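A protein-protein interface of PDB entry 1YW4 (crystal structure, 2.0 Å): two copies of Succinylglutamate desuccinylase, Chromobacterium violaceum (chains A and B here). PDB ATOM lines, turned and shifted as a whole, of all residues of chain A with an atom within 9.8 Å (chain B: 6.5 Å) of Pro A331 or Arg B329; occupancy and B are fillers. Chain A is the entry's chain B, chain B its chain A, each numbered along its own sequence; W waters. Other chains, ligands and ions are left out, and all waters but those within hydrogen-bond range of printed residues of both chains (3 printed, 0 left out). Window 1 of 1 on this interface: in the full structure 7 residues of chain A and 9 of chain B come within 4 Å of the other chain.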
ATOM      1  N   TYR A 163      23.503 -19.304 -20.504  1.00  0.00           N
ATOM      2  CA  TYR A 163      23.242 -17.870 -20.564  1.00  0.00           C
ATOM      3  C   TYR A 163      24.412 -16.987 -20.992  1.00  0.00           C
ATOM      4  O   TYR A 163      25.375 -16.818 -20.254  1.00  0.00           O
ATOM      5  CB  TYR A 163      22.733 -17.419 -19.180  1.00  0.00           C
ATOM      6  CG  TYR A 163      22.230 -15.992 -19.063  1.00  0.00           C
ATOM      7  CD1 TYR A 163      21.739 -15.510 -17.848  1.00  0.00           C
ATOM      8  CD2 TYR A 163      22.214 -15.137 -20.162  1.00  0.00           C
ATOM      9  CE1 TYR A 163      21.241 -14.212 -17.734  1.00  0.00           C
ATOM     10  CE2 TYR A 163      21.721 -13.843 -20.058  1.00  0.00           C
ATOM     11  CZ  TYR A 163      21.233 -13.386 -18.848  1.00  0.00           C
ATOM     12  OH  TYR A 163      20.712 -12.117 -18.766  1.00  0.00           O
ATOM     13  N   PHE A 165      26.071 -14.229 -20.748  1.00  0.00           N
ATOM     14  CA  PHE A 165      26.111 -13.052 -19.871  1.00  0.00           C
ATOM     15  C   PHE A 165      27.054 -12.010 -20.479  1.00  0.00           C
ATOM     16  O   PHE A 165      28.254 -12.252 -20.597  1.00  0.00           O
ATOM     17  CB  PHE A 165      26.615 -13.459 -18.475  1.00  0.00           C
ATOM     18  CG  PHE A 165      26.008 -12.669 -17.344  1.00  0.00           C
ATOM     19  CD1 PHE A 165      24.673 -12.847 -16.996  1.00  0.00           C
ATOM     20  CD2 PHE A 165      26.772 -11.749 -16.625  1.00  0.00           C
ATOM     21  CE1 PHE A 165      24.104 -12.124 -15.950  1.00  0.00           C
ATOM     22  CE2 PHE A 165      26.213 -11.017 -15.573  1.00  0.00           C
ATOM     23  CZ  PHE A 165      24.873 -11.204 -15.233  1.00  0.00           C
ATOM     24  N   LEU A 166      26.526 -10.850 -20.859  1.00  0.00           N
ATOM     25  CA  LEU A 166      27.367  -9.825 -21.472  1.00  0.00           C
ATOM     26  C   LEU A 166      27.224  -8.450 -20.809  1.00  0.00           C
ATOM     27  O   LEU A 166      26.185  -8.133 -20.227  1.00  0.00           O
ATOM     28  CB  LEU A 166      27.041  -9.731 -22.968  1.00  0.00           C
ATOM     29  CG  LEU A 166      26.973 -11.068 -23.723  1.00  0.00           C
ATOM     30  CD1 LEU A 166      26.537 -10.825 -25.164  1.00  0.00           C
ATOM     31  CD2 LEU A 166      28.327 -11.764 -23.684  1.00  0.00           C
ATOM     32  N   HIS A 167      28.274  -7.638 -20.902  1.00  0.00           N
ATOM     33  CA  HIS A 167      28.272  -6.299 -20.312  1.00  0.00           C
ATOM     34  C   HIS A 167      27.948  -6.275 -18.813  1.00  0.00           C
ATOM     35  O   HIS A 167      27.147  -5.460 -18.355  1.00  0.00           O
ATOM     36  CB  HIS A 167      27.288  -5.399 -21.063  1.00  0.00           C
ATOM     37  CG  HIS A 167      27.738  -5.040 -22.445  1.00  0.00           C
ATOM     38  ND1 HIS A 167      28.920  -4.374 -22.691  1.00  0.00           N
ATOM     39  CD2 HIS A 167      27.166  -5.250 -23.654  1.00  0.00           C
ATOM     40  CE1 HIS A 167      29.057  -4.189 -23.991  1.00  0.00           C
ATOM     41  NE2 HIS A 167      28.006  -4.711 -24.600  1.00  0.00           N
ATOM     42  N   ASP A 168      28.576  -7.173 -18.058  1.00  0.00           N
ATOM     43  CA  ASP A 168      28.382  -7.259 -16.610  1.00  0.00           C
ATOM     44  C   ASP A 168      26.908  -7.369 -16.214  1.00  0.00           C
ATOM     45  O   ASP A 168      26.546  -7.111 -15.063  1.00  0.00           O
ATOM     46  CB  ASP A 168      29.003  -6.033 -15.930  1.00  0.00           C
ATOM     47  CG  ASP A 168      29.914  -6.402 -14.766  1.00  0.00           C
ATOM     48  OD1 ASP A 168      29.474  -7.155 -13.874  1.00  0.00           O
ATOM     49  OD2 ASP A 168      31.072  -5.930 -14.741  1.00  0.00           O
ATOM     50  N   GLY A 169      26.062  -7.744 -17.171  1.00  0.00           N
ATOM     51  CA  GLY A 169      24.643  -7.883 -16.898  1.00  0.00           C
ATOM     52  C   GLY A 169      23.921  -6.556 -16.750  1.00  0.00           C
ATOM     53  O   GLY A 169      22.971  -6.439 -15.975  1.00  0.00           O
ATOM     54  N   ARG A 170      24.366  -5.551 -17.495  1.00  0.00           N
ATOM     55  CA  ARG A 170      23.747  -4.235 -17.433  1.00  0.00           C
ATOM     56  C   ARG A 170      22.322  -4.291 -17.965  1.00  0.00           C
ATOM     57  O   ARG A 170      21.478  -3.482 -17.584  1.00  0.00           O
ATOM     58  CB  ARG A 170      24.580  -3.230 -18.231  1.00  0.00           C
ATOM     59  CG  ARG A 170      25.959  -3.017 -17.636  1.00  0.00           C
ATOM     60  CD  ARG A 170      26.933  -2.416 -18.629  1.00  0.00           C
ATOM     61  NE  ARG A 170      28.311  -2.570 -18.170  1.00  0.00           N
ATOM     62  CZ  ARG A 170      29.381  -2.244 -18.890  1.00  0.00           C
ATOM     63  NH1 ARG A 170      30.601  -2.421 -18.394  1.00  0.00           N
ATOM     64  NH2 ARG A 170      29.233  -1.741 -20.107  1.00  0.00           N
ATOM     65  N   THR A 171      22.057  -5.256 -18.840  1.00  0.00           N
ATOM     66  CA  THR A 171      20.723  -5.427 -19.412  1.00  0.00           C
ATOM     67  C   THR A 171      20.132  -6.751 -18.941  1.00  0.00           C
ATOM     68  O   THR A 171      19.227  -7.303 -19.567  1.00  0.00           O
ATOM     69  CB  THR A 171      20.763  -5.430 -20.956  1.00  0.00           C
ATOM     70  OG1 THR A 171      19.437  -5.619 -21.463  1.00  0.00           O
ATOM     71  CG2 THR A 171      21.657  -6.551 -21.472  1.00  0.00           C
ATOM     72  N   HIS A 172      20.654  -7.256 -17.830  1.00  0.00           N
ATOM     73  CA  HIS A 172      20.199  -8.522 -17.276  1.00  0.00           C
ATOM     74  C   HIS A 172      18.789  -8.464 -16.679  1.00  0.00           C
ATOM     75  O   HIS A 172      18.406  -7.477 -16.048  1.00  0.00           O
ATOM     76  CB  HIS A 172      21.195  -8.998 -16.222  1.00  0.00           C
ATOM     77  CG  HIS A 172      20.711 -10.163 -15.424  1.00  0.00           C
ATOM     78  ND1 HIS A 172      20.305 -11.344 -16.006  1.00  0.00           N
ATOM     79  CD2 HIS A 172      20.549 -10.324 -14.090  1.00  0.00           C
ATOM     80  CE1 HIS A 172      19.914 -12.183 -15.065  1.00  0.00           C
ATOM     81  NE2 HIS A 172      20.052 -11.588 -13.892  1.00  0.00           N
ATOM     82  N   LEU A 177      15.436 -15.356 -15.383  1.00  0.00           N
ATOM     83  CA  LEU A 177      15.962 -16.483 -14.617  1.00  0.00           C
ATOM     84  C   LEU A 177      14.799 -17.088 -13.832  1.00  0.00           C
ATOM     85  O   LEU A 177      14.759 -18.295 -13.590  1.00  0.00           O
ATOM     86  CB  LEU A 177      17.073 -16.003 -13.674  1.00  0.00           C
ATOM     87  CG  LEU A 177      18.473 -16.607 -13.876  1.00  0.00           C
ATOM     88  CD1 LEU A 177      18.804 -16.705 -15.357  1.00  0.00           C
ATOM     89  CD2 LEU A 177      19.517 -15.751 -13.149  1.00  0.00           C
ATOM     90  N   LEU A 190      26.497 -19.676 -16.947  1.00  0.00           N
ATOM     91  CA  LEU A 190      26.802 -18.317 -17.368  1.00  0.00           C
ATOM     92  C   LEU A 190      28.169 -18.255 -18.044  1.00  0.00           C
ATOM     93  O   LEU A 190      29.133 -18.830 -17.548  1.00  0.00           O
ATOM     94  CB  LEU A 190      26.833 -17.388 -16.150  1.00  0.00           C
ATOM     95  CG  LEU A 190      25.619 -17.395 -15.215  1.00  0.00           C
ATOM     96  CD1 LEU A 190      25.865 -16.441 -14.057  1.00  0.00           C
ATOM     97  CD2 LEU A 190      24.382 -16.999 -15.978  1.00  0.00           C
ATOM     98  N   THR A 192      30.693 -15.303 -20.260  1.00  0.00           N
ATOM     99  CA  THR A 192      30.837 -13.942 -20.776  1.00  0.00           C
ATOM    100  C   THR A 192      31.662 -13.919 -22.046  1.00  0.00           C
ATOM    101  O   THR A 192      31.549 -12.995 -22.850  1.00  0.00           O
ATOM    102  CB  THR A 192      31.527 -13.022 -19.756  1.00  0.00           C
ATOM    103  OG1 THR A 192      30.876 -13.138 -18.484  1.00  0.00           O
ATOM    104  CG2 THR A 192      31.457 -11.572 -20.228  1.00  0.00           C
ATOM    105  N   GLU A 252      16.132 -18.111  -5.806  1.00  0.00           N
ATOM    106  CA  GLU A 252      17.499 -18.459  -6.160  1.00  0.00           C
ATOM    107  C   GLU A 252      18.022 -19.688  -5.434  1.00  0.00           C
ATOM    108  O   GLU A 252      18.903 -20.390  -5.937  1.00  0.00           O
ATOM    109  CB  GLU A 252      18.404 -17.253  -5.900  1.00  0.00           C
ATOM    110  CG  GLU A 252      17.955 -16.402  -4.727  1.00  0.00           C
ATOM    111  CD  GLU A 252      18.598 -15.033  -4.734  1.00  0.00           C
ATOM    112  OE1 GLU A 252      19.844 -14.958  -4.632  1.00  0.00           O
ATOM    113  OE2 GLU A 252      17.855 -14.030  -4.845  1.00  0.00           O
ATOM    114  N   LEU A 257      23.693 -21.541 -10.160  1.00  0.00           N
ATOM    115  CA  LEU A 257      24.368 -20.908 -11.281  1.00  0.00           C
ATOM    116  C   LEU A 257      25.809 -21.381 -11.346  1.00  0.00           C
ATOM    117  O   LEU A 257      26.479 -21.517 -10.316  1.00  0.00           O
ATOM    118  CB  LEU A 257      24.344 -19.380 -11.130  1.00  0.00           C
ATOM    119  CG  LEU A 257      22.969 -18.709 -10.994  1.00  0.00           C
ATOM    120  CD1 LEU A 257      23.150 -17.218 -10.815  1.00  0.00           C
ATOM    121  CD2 LEU A 257      22.124 -19.000 -12.227  1.00  0.00           C
ATOM    122  N   ARG A 259      29.679 -21.319 -13.830  1.00  0.00           N
ATOM    123  CA  ARG A 259      30.516 -20.600 -14.787  1.00  0.00           C
ATOM    124  C   ARG A 259      31.727 -21.469 -15.103  1.00  0.00           C
ATOM    125  O   ARG A 259      32.140 -22.296 -14.285  1.00  0.00           O
ATOM    126  CB  ARG A 259      30.993 -19.263 -14.202  1.00  0.00           C
ATOM    127  CG  ARG A 259      31.973 -19.391 -13.039  1.00  0.00           C
ATOM    128  CD  ARG A 259      32.329 -18.023 -12.466  1.00  0.00           C
ATOM    129  NE  ARG A 259      32.962 -17.161 -13.461  1.00  0.00           N
ATOM    130  CZ  ARG A 259      34.166 -17.375 -13.983  1.00  0.00           C
ATOM    131  NH1 ARG A 259      34.658 -16.536 -14.887  1.00  0.00           N
ATOM    132  NH2 ARG A 259      34.884 -18.419 -13.593  1.00  0.00           N
ATOM    133  N   GLU A 305      34.009 -28.974  -5.784  1.00  0.00           N
ATOM    134  CA  GLU A 305      32.783 -28.323  -6.248  1.00  0.00           C
ATOM    135  C   GLU A 305      32.806 -28.075  -7.751  1.00  0.00           C
ATOM    136  O   GLU A 305      31.854 -27.537  -8.311  1.00  0.00           O
ATOM    137  CB  GLU A 305      32.551 -27.001  -5.509  1.00  0.00           C
ATOM    138  CG  GLU A 305      32.136 -27.169  -4.053  1.00  0.00           C
ATOM    139  CD  GLU A 305      31.701 -25.865  -3.399  1.00  0.00           C
ATOM    140  OE1 GLU A 305      31.289 -25.905  -2.217  1.00  0.00           O
ATOM    141  OE2 GLU A 305      31.770 -24.804  -4.062  1.00  0.00           O
ATOM    142  N   GLU A 326      32.331 -24.125 -12.237  1.00  0.00           N
ATOM    143  CA  GLU A 326      32.275 -23.902 -10.792  1.00  0.00           C
ATOM    144  C   GLU A 326      31.028 -23.108 -10.440  1.00  0.00           C
ATOM    145  O   GLU A 326      30.400 -22.498 -11.313  1.00  0.00           O
ATOM    146  CB  GLU A 326      33.510 -23.114 -10.335  1.00  0.00           C
ATOM    147  CG  GLU A 326      33.607 -21.727 -10.953  1.00  0.00           C
ATOM    148  CD  GLU A 326      34.867 -20.968 -10.553  1.00  0.00           C
ATOM    149  OE1 GLU A 326      35.241 -20.028 -11.292  1.00  0.00           O
ATOM    150  OE2 GLU A 326      35.474 -21.297  -9.506  1.00  0.00           O
ATOM    151  N   PRO A 327      30.638 -23.114  -9.154  1.00  0.00           N
ATOM    152  CA  PRO A 327      29.451 -22.362  -8.754  1.00  0.00           C
ATOM    153  C   PRO A 327      29.693 -20.883  -9.009  1.00  0.00           C
ATOM    154  O   PRO A 327      30.798 -20.377  -8.786  1.00  0.00           O
ATOM    155  CB  PRO A 327      29.311 -22.694  -7.270  1.00  0.00           C
ATOM    156  CG  PRO A 327      30.725 -23.012  -6.851  1.00  0.00           C
ATOM    157  CD  PRO A 327      31.213 -23.835  -8.004  1.00  0.00           C
ATOM    158  N   ALA A 328      28.662 -20.200  -9.492  1.00  0.00           N
ATOM    159  CA  ALA A 328      28.768 -18.781  -9.800  1.00  0.00           C
ATOM    160  C   ALA A 328      27.752 -17.954  -9.038  1.00  0.00           C
ATOM    161  O   ALA A 328      26.802 -18.481  -8.467  1.00  0.00           O
ATOM    162  CB  ALA A 328      28.588 -18.564 -11.302  1.00  0.00           C
ATOM    163  N   ARG A 329      27.974 -16.645  -9.031  1.00  0.00           N
ATOM    164  CA  ARG A 329      27.076 -15.712  -8.375  1.00  0.00           C
ATOM    165  C   ARG A 329      26.945 -14.477  -9.253  1.00  0.00           C
ATOM    166  O   ARG A 329      27.891 -14.097  -9.953  1.00  0.00           O
ATOM    167  CB  ARG A 329      27.617 -15.307  -7.004  1.00  0.00           C
ATOM    168  CG  ARG A 329      27.726 -16.449  -6.016  1.00  0.00           C
ATOM    169  CD  ARG A 329      27.184 -16.035  -4.660  1.00  0.00           C
ATOM    170  NE  ARG A 329      27.768 -14.782  -4.181  1.00  0.00           N
ATOM    171  CZ  ARG A 329      27.371 -14.155  -3.078  1.00  0.00           C
ATOM    172  NH1 ARG A 329      27.949 -13.023  -2.711  1.00  0.00           N
ATOM    173  NH2 ARG A 329      26.393 -14.662  -2.340  1.00  0.00           N
ATOM    174  N   LEU A 330      25.769 -13.859  -9.218  1.00  0.00           N
ATOM    175  CA  LEU A 330      25.515 -12.659 -10.005  1.00  0.00           C
ATOM    176  C   LEU A 330      26.277 -11.475  -9.410  1.00  0.00           C
ATOM    177  O   LEU A 330      26.459 -11.390  -8.196  1.00  0.00           O
ATOM    178  CB  LEU A 330      24.011 -12.357 -10.039  1.00  0.00           C
ATOM    179  CG  LEU A 330      23.126 -13.353 -10.799  1.00  0.00           C
ATOM    180  CD1 LEU A 330      21.669 -12.923 -10.709  1.00  0.00           C
ATOM    181  CD2 LEU A 330      23.563 -13.423 -12.247  1.00  0.00           C
ATOM    182  N   PRO A 331      26.732 -10.575 -10.276  1.00  0.00           N
ATOM    183  CA  PRO A 331      27.472  -9.395  -9.845  1.00  0.00           C
ATOM    184  C   PRO A 331      27.270  -8.270 -10.847  1.00  0.00           C
ATOM    185  O   PRO A 331      26.587  -8.518 -11.864  1.00  0.00           O
ATOM    186  CB  PRO A 331      28.955  -9.725  -9.726  1.00  0.00           C
ATOM    187  N   LEU B 190      43.266 -14.754  -2.323  1.00  0.00           N
ATOM    188  CA  LEU B 190      43.027 -16.109  -1.829  1.00  0.00           C
ATOM    189  C   LEU B 190      43.864 -17.077  -2.661  1.00  0.00           C
ATOM    190  O   LEU B 190      43.660 -17.201  -3.872  1.00  0.00           O
ATOM    191  CB  LEU B 190      41.545 -16.464  -1.973  1.00  0.00           C
ATOM    192  CG  LEU B 190      40.512 -15.372  -1.642  1.00  0.00           C
ATOM    193  CD1 LEU B 190      39.131 -15.829  -2.118  1.00  0.00           C
ATOM    194  CD2 LEU B 190      40.501 -15.077  -0.152  1.00  0.00           C
ATOM    195  N   GLU B 252      31.400  -7.695   2.675  1.00  0.00           N
ATOM    196  CA  GLU B 252      32.156  -8.191   1.537  1.00  0.00           C
ATOM    197  C   GLU B 252      32.087  -7.295   0.307  1.00  0.00           C
ATOM    198  O   GLU B 252      32.884  -7.446  -0.617  1.00  0.00           O
ATOM    199  CB  GLU B 252      31.701  -9.611   1.183  1.00  0.00           C
ATOM    200  CG  GLU B 252      30.263  -9.732   0.729  1.00  0.00           C
ATOM    201  CD  GLU B 252      29.891 -11.167   0.382  1.00  0.00           C
ATOM    202  OE1 GLU B 252      29.855 -12.014   1.298  1.00  0.00           O
ATOM    203  OE2 GLU B 252      29.638 -11.451  -0.809  1.00  0.00           O
ATOM    204  N   ASP B 253      31.146  -6.355   0.299  1.00  0.00           N
ATOM    205  CA  ASP B 253      31.001  -5.441  -0.831  1.00  0.00           C
ATOM    206  C   ASP B 253      32.033  -4.319  -0.759  1.00  0.00           C
ATOM    207  O   ASP B 253      32.125  -3.487  -1.662  1.00  0.00           O
ATOM    208  CB  ASP B 253      29.591  -4.839  -0.861  1.00  0.00           C
ATOM    209  CG  ASP B 253      28.513  -5.887  -1.062  1.00  0.00           C
ATOM    210  OD1 ASP B 253      28.612  -6.665  -2.037  1.00  0.00           O
ATOM    211  OD2 ASP B 253      27.563  -5.930  -0.246  1.00  0.00           O
ATOM    212  N   LEU B 257      38.053  -9.422  -3.171  1.00  0.00           N
ATOM    213  CA  LEU B 257      38.869 -10.624  -3.075  1.00  0.00           C
ATOM    214  C   LEU B 257      39.339 -11.009  -4.475  1.00  0.00           C
ATOM    215  O   LEU B 257      38.656 -10.733  -5.465  1.00  0.00           O
ATOM    216  CB  LEU B 257      38.054 -11.775  -2.481  1.00  0.00           C
ATOM    217  CG  LEU B 257      37.305 -11.515  -1.169  1.00  0.00           C
ATOM    218  CD1 LEU B 257      36.431 -12.725  -0.863  1.00  0.00           C
ATOM    219  CD2 LEU B 257      38.276 -11.263  -0.019  1.00  0.00           C
ATOM    220  N   PHE B 258      40.498 -11.653  -4.551  1.00  0.00           N
ATOM    221  CA  PHE B 258      41.055 -12.072  -5.829  1.00  0.00           C
ATOM    222  C   PHE B 258      41.719 -13.443  -5.743  1.00  0.00           C
ATOM    223  O   PHE B 258      42.057 -13.920  -4.664  1.00  0.00           O
ATOM    224  CB  PHE B 258      42.093 -11.054  -6.324  1.00  0.00           C
ATOM    225  CG  PHE B 258      41.556  -9.652  -6.488  1.00  0.00           C
ATOM    226  CD1 PHE B 258      41.501  -8.774  -5.407  1.00  0.00           C
ATOM    227  CD2 PHE B 258      41.096  -9.216  -7.727  1.00  0.00           C
ATOM    228  CE1 PHE B 258      40.993  -7.471  -5.555  1.00  0.00           C
ATOM    229  CE2 PHE B 258      40.587  -7.918  -7.891  1.00  0.00           C
ATOM    230  CZ  PHE B 258      40.536  -7.048  -6.802  1.00  0.00           C
ATOM    231  N   ARG B 259      41.894 -14.074  -6.896  1.00  0.00           N
ATOM    232  CA  ARG B 259      42.559 -15.361  -6.972  1.00  0.00           C
ATOM    233  C   ARG B 259      43.353 -15.346  -8.269  1.00  0.00           C
ATOM    234  O   ARG B 259      43.038 -14.591  -9.198  1.00  0.00           O
ATOM    235  CB  ARG B 259      41.542 -16.509  -6.985  1.00  0.00           C
ATOM    236  CG  ARG B 259      40.713 -16.584  -8.255  1.00  0.00           C
ATOM    237  CD  ARG B 259      39.707 -17.718  -8.202  1.00  0.00           C
ATOM    238  NE  ARG B 259      39.031 -17.888  -9.487  1.00  0.00           N
ATOM    239  CZ  ARG B 259      37.987 -18.688  -9.682  1.00  0.00           C
ATOM    240  NH1 ARG B 259      37.493 -19.393  -8.673  1.00  0.00           N
ATOM    241  NH2 ARG B 259      37.441 -18.785 -10.888  1.00  0.00           N
ATOM    242  N   PRO B 327      38.761 -11.262  -9.976  1.00  0.00           N
ATOM    243  CA  PRO B 327      37.882 -11.139  -8.809  1.00  0.00           C
ATOM    244  C   PRO B 327      37.476 -12.510  -8.269  1.00  0.00           C
ATOM    245  O   PRO B 327      37.281 -13.456  -9.032  1.00  0.00           O
ATOM    246  CB  PRO B 327      36.685 -10.362  -9.362  1.00  0.00           C
ATOM    247  CG  PRO B 327      37.307  -9.493 -10.427  1.00  0.00           C
ATOM    248  CD  PRO B 327      38.254 -10.461 -11.107  1.00  0.00           C
ATOM    249  N   ALA B 328      37.366 -12.613  -6.951  1.00  0.00           N
ATOM    250  CA  ALA B 328      36.980 -13.863  -6.312  1.00  0.00           C
ATOM    251  C   ALA B 328      35.767 -13.606  -5.433  1.00  0.00           C
ATOM    252  O   ALA B 328      35.733 -12.639  -4.675  1.00  0.00           O
ATOM    253  CB  ALA B 328      38.132 -14.417  -5.474  1.00  0.00           C
ATOM    254  N   ARG B 329      34.771 -14.473  -5.548  1.00  0.00           N
ATOM    255  CA  ARG B 329      33.551 -14.335  -4.769  1.00  0.00           C
ATOM    256  C   ARG B 329      33.446 -15.475  -3.765  1.00  0.00           C
ATOM    257  O   ARG B 329      33.819 -16.607  -4.065  1.00  0.00           O
ATOM    258  CB  ARG B 329      32.333 -14.352  -5.702  1.00  0.00           C
ATOM    259  CG  ARG B 329      32.345 -13.282  -6.798  1.00  0.00           C
ATOM    260  CD  ARG B 329      32.195 -11.875  -6.233  1.00  0.00           C
ATOM    261  NE  ARG B 329      30.921 -11.679  -5.542  1.00  0.00           N
ATOM    262  CZ  ARG B 329      29.731 -11.662  -6.139  1.00  0.00           C
ATOM    263  NH1 ARG B 329      29.632 -11.829  -7.449  1.00  0.00           N
ATOM    264  NH2 ARG B 329      28.632 -11.477  -5.420  1.00  0.00           N
ATOM    265  N   LEU B 330      32.959 -15.167  -2.568  1.00  0.00           N
ATOM    266  CA  LEU B 330      32.776 -16.176  -1.528  1.00  0.00           C
ATOM    267  C   LEU B 330      31.459 -16.905  -1.800  1.00  0.00           C
ATOM    268  O   LEU B 330      30.606 -16.399  -2.529  1.00  0.00           O
ATOM    269  CB  LEU B 330      32.721 -15.511  -0.148  1.00  0.00           C
ATOM    270  CG  LEU B 330      34.031 -14.974   0.436  1.00  0.00           C
ATOM    271  CD1 LEU B 330      33.737 -14.126   1.666  1.00  0.00           C
ATOM    272  CD2 LEU B 330      34.952 -16.141   0.789  1.00  0.00           C
ATOM    273  N   PRO B 331      31.277 -18.104  -1.223  1.00  0.00           N
ATOM    274  CA  PRO B 331      30.039 -18.869  -1.430  1.00  0.00           C
ATOM    275  C   PRO B 331      28.818 -18.121  -0.898  1.00  0.00           C
ATOM    276  O   PRO B 331      27.708 -18.270  -1.410  1.00  0.00           O
ATOM    277  CB  PRO B 331      30.306 -20.170  -0.672  1.00  0.00           C
ATOM    278  CG  PRO B 331      31.204 -19.728   0.440  1.00  0.00           C
ATOM    279  CD  PRO B 331      32.167 -18.797  -0.276  1.00  0.00           C
ATOM    280  N   SER B 332      29.035 -17.309   0.132  1.00  0.00           N
ATOM    281  CA  SER B 332      27.956 -16.527   0.726  1.00  0.00           C
ATOM    282  C   SER B 332      28.454 -15.148   1.149  1.00  0.00           C
ATOM    283  O   SER B 332      29.443 -14.673   0.550  1.00  0.00           O
ATOM    284  CB  SER B 332      27.349 -17.270   1.927  1.00  0.00           C
ATOM    285  OG  SER B 332      26.616 -18.413   1.507  1.00  0.00           O
HETATM  286  O   HOH W   1      26.280 -13.222   0.614  1.00  0.00           O
HETATM  287  O   HOH W   2      30.985 -13.105  -9.618  1.00  0.00           O
HETATM  288  O   HOH W   3      25.580 -12.259  -5.298  1.00  0.00           O
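Water W2 lies within hydrogen-bond range of the guanidinium group (NH1) of Arg B329 (2.9 Å) and the backbone carbonyl oxygen (O) of Arg A329 (3.3 Å). Water W3 lies within hydrogen-bond range of O of Leu A330 (3.2 Å) and NH2 of Arg B329 (3.2 Å). Water W1 bridges the guanidinium group (NH2) of Arg A329 and the backbone carbonyl oxygen (O) of Ser B332.
Of chain B, only Arg B329 comes within 4 Å of Pro A331. Arg B329 touches just these residues of chain A: Arg A329 (3.2 Å), Leu A330 (3.3 Å) and Pro A331 (3.2 Å). Of chain A, only Arg A329 comes within 4 Å of Leu B330. Printed residues of chain A within 4 Å of Pro B331: Arg A329. Printed residues of chain A within 4 Å of Arg B259: Arg A259 (3.7 Å) and Glu A326 (2.6 Å). Of the printed residues of chain B, Arg A259 touches Arg B259. Printed residues of chain B within 4 Å of Leu A330: Arg B329. Printed residues of chain B within 4 Å of Arg A329: Glu B252, Arg B329, Leu B330, Pro B331 and Ser B332. His A172 touches none of the printed residues of chain B. The nearest printed residue of chain A that does not touch Glu B252 is Leu A330 (8.0 Å).
NH2 of Arg A259 is in salt-bridge range of OE1 of Glu A326, at 2.8 Å.
Among the printed residues, pairs that only touch across the chains: Arg A259 with Arg B259 (3.7 Å), Arg A329 with Leu B330 (3.7 Å), Arg A329 with Pro B331 (3.95 Å), Arg A329 with Ser B332 (3.9 Å) and Pro A331 with Arg B329 (3.2 Å).
Arg A259 touches its own counterpart, Arg B259. Arg A329 touches Glu B252, but with the chains exchanged Glu A252 does not touch Arg B329 (9.5 Å). Arg A329 touches Leu B330, and with the chains exchanged Leu A330 touches Arg B329. Arg A329 touches Pro B331, and with the chains exchanged Pro A331 touches Arg B329. Positions printed for both chains: 190, 252, 257, 259, 327, 328, 329, 330 and 331.
NH2 of Arg B329 lies close to NH1 of Arg A329, 3.2 Å away. The side-chain carboxylate of Glu B252 is in salt-bridge range of the guanidinium group of Arg A329, 3.0 Å away. NH2 of Arg B259 is in salt-bridge range of OE1 of Glu A326, at 2.6 Å. The guanidinium group (NH1) of Arg B329 sits at hydrogen-bond distance from the backbone carbonyl oxygen (O) of Leu A330, 3.3 Å away.
Hydrophobic or aromatic side chains of chain A within 4 Å of the printed part of chain B: Pro A331. Along chain A the printed residues that touch a printed residue of chain B span positions 259 to 331. Printed residues of chain B that touch a printed residue of chain A: Glu B252, Arg B259, Arg B329, Leu B330, Pro B331 and Ser B332. Among the printed residues, Asp or Glu carboxylates within 4 Å of a Lys or Arg side-chain nitrogen of the other chain: Glu A326 with Arg B259 (2.6 Å) and Arg A329 with Glu B252 (3.0 Å).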
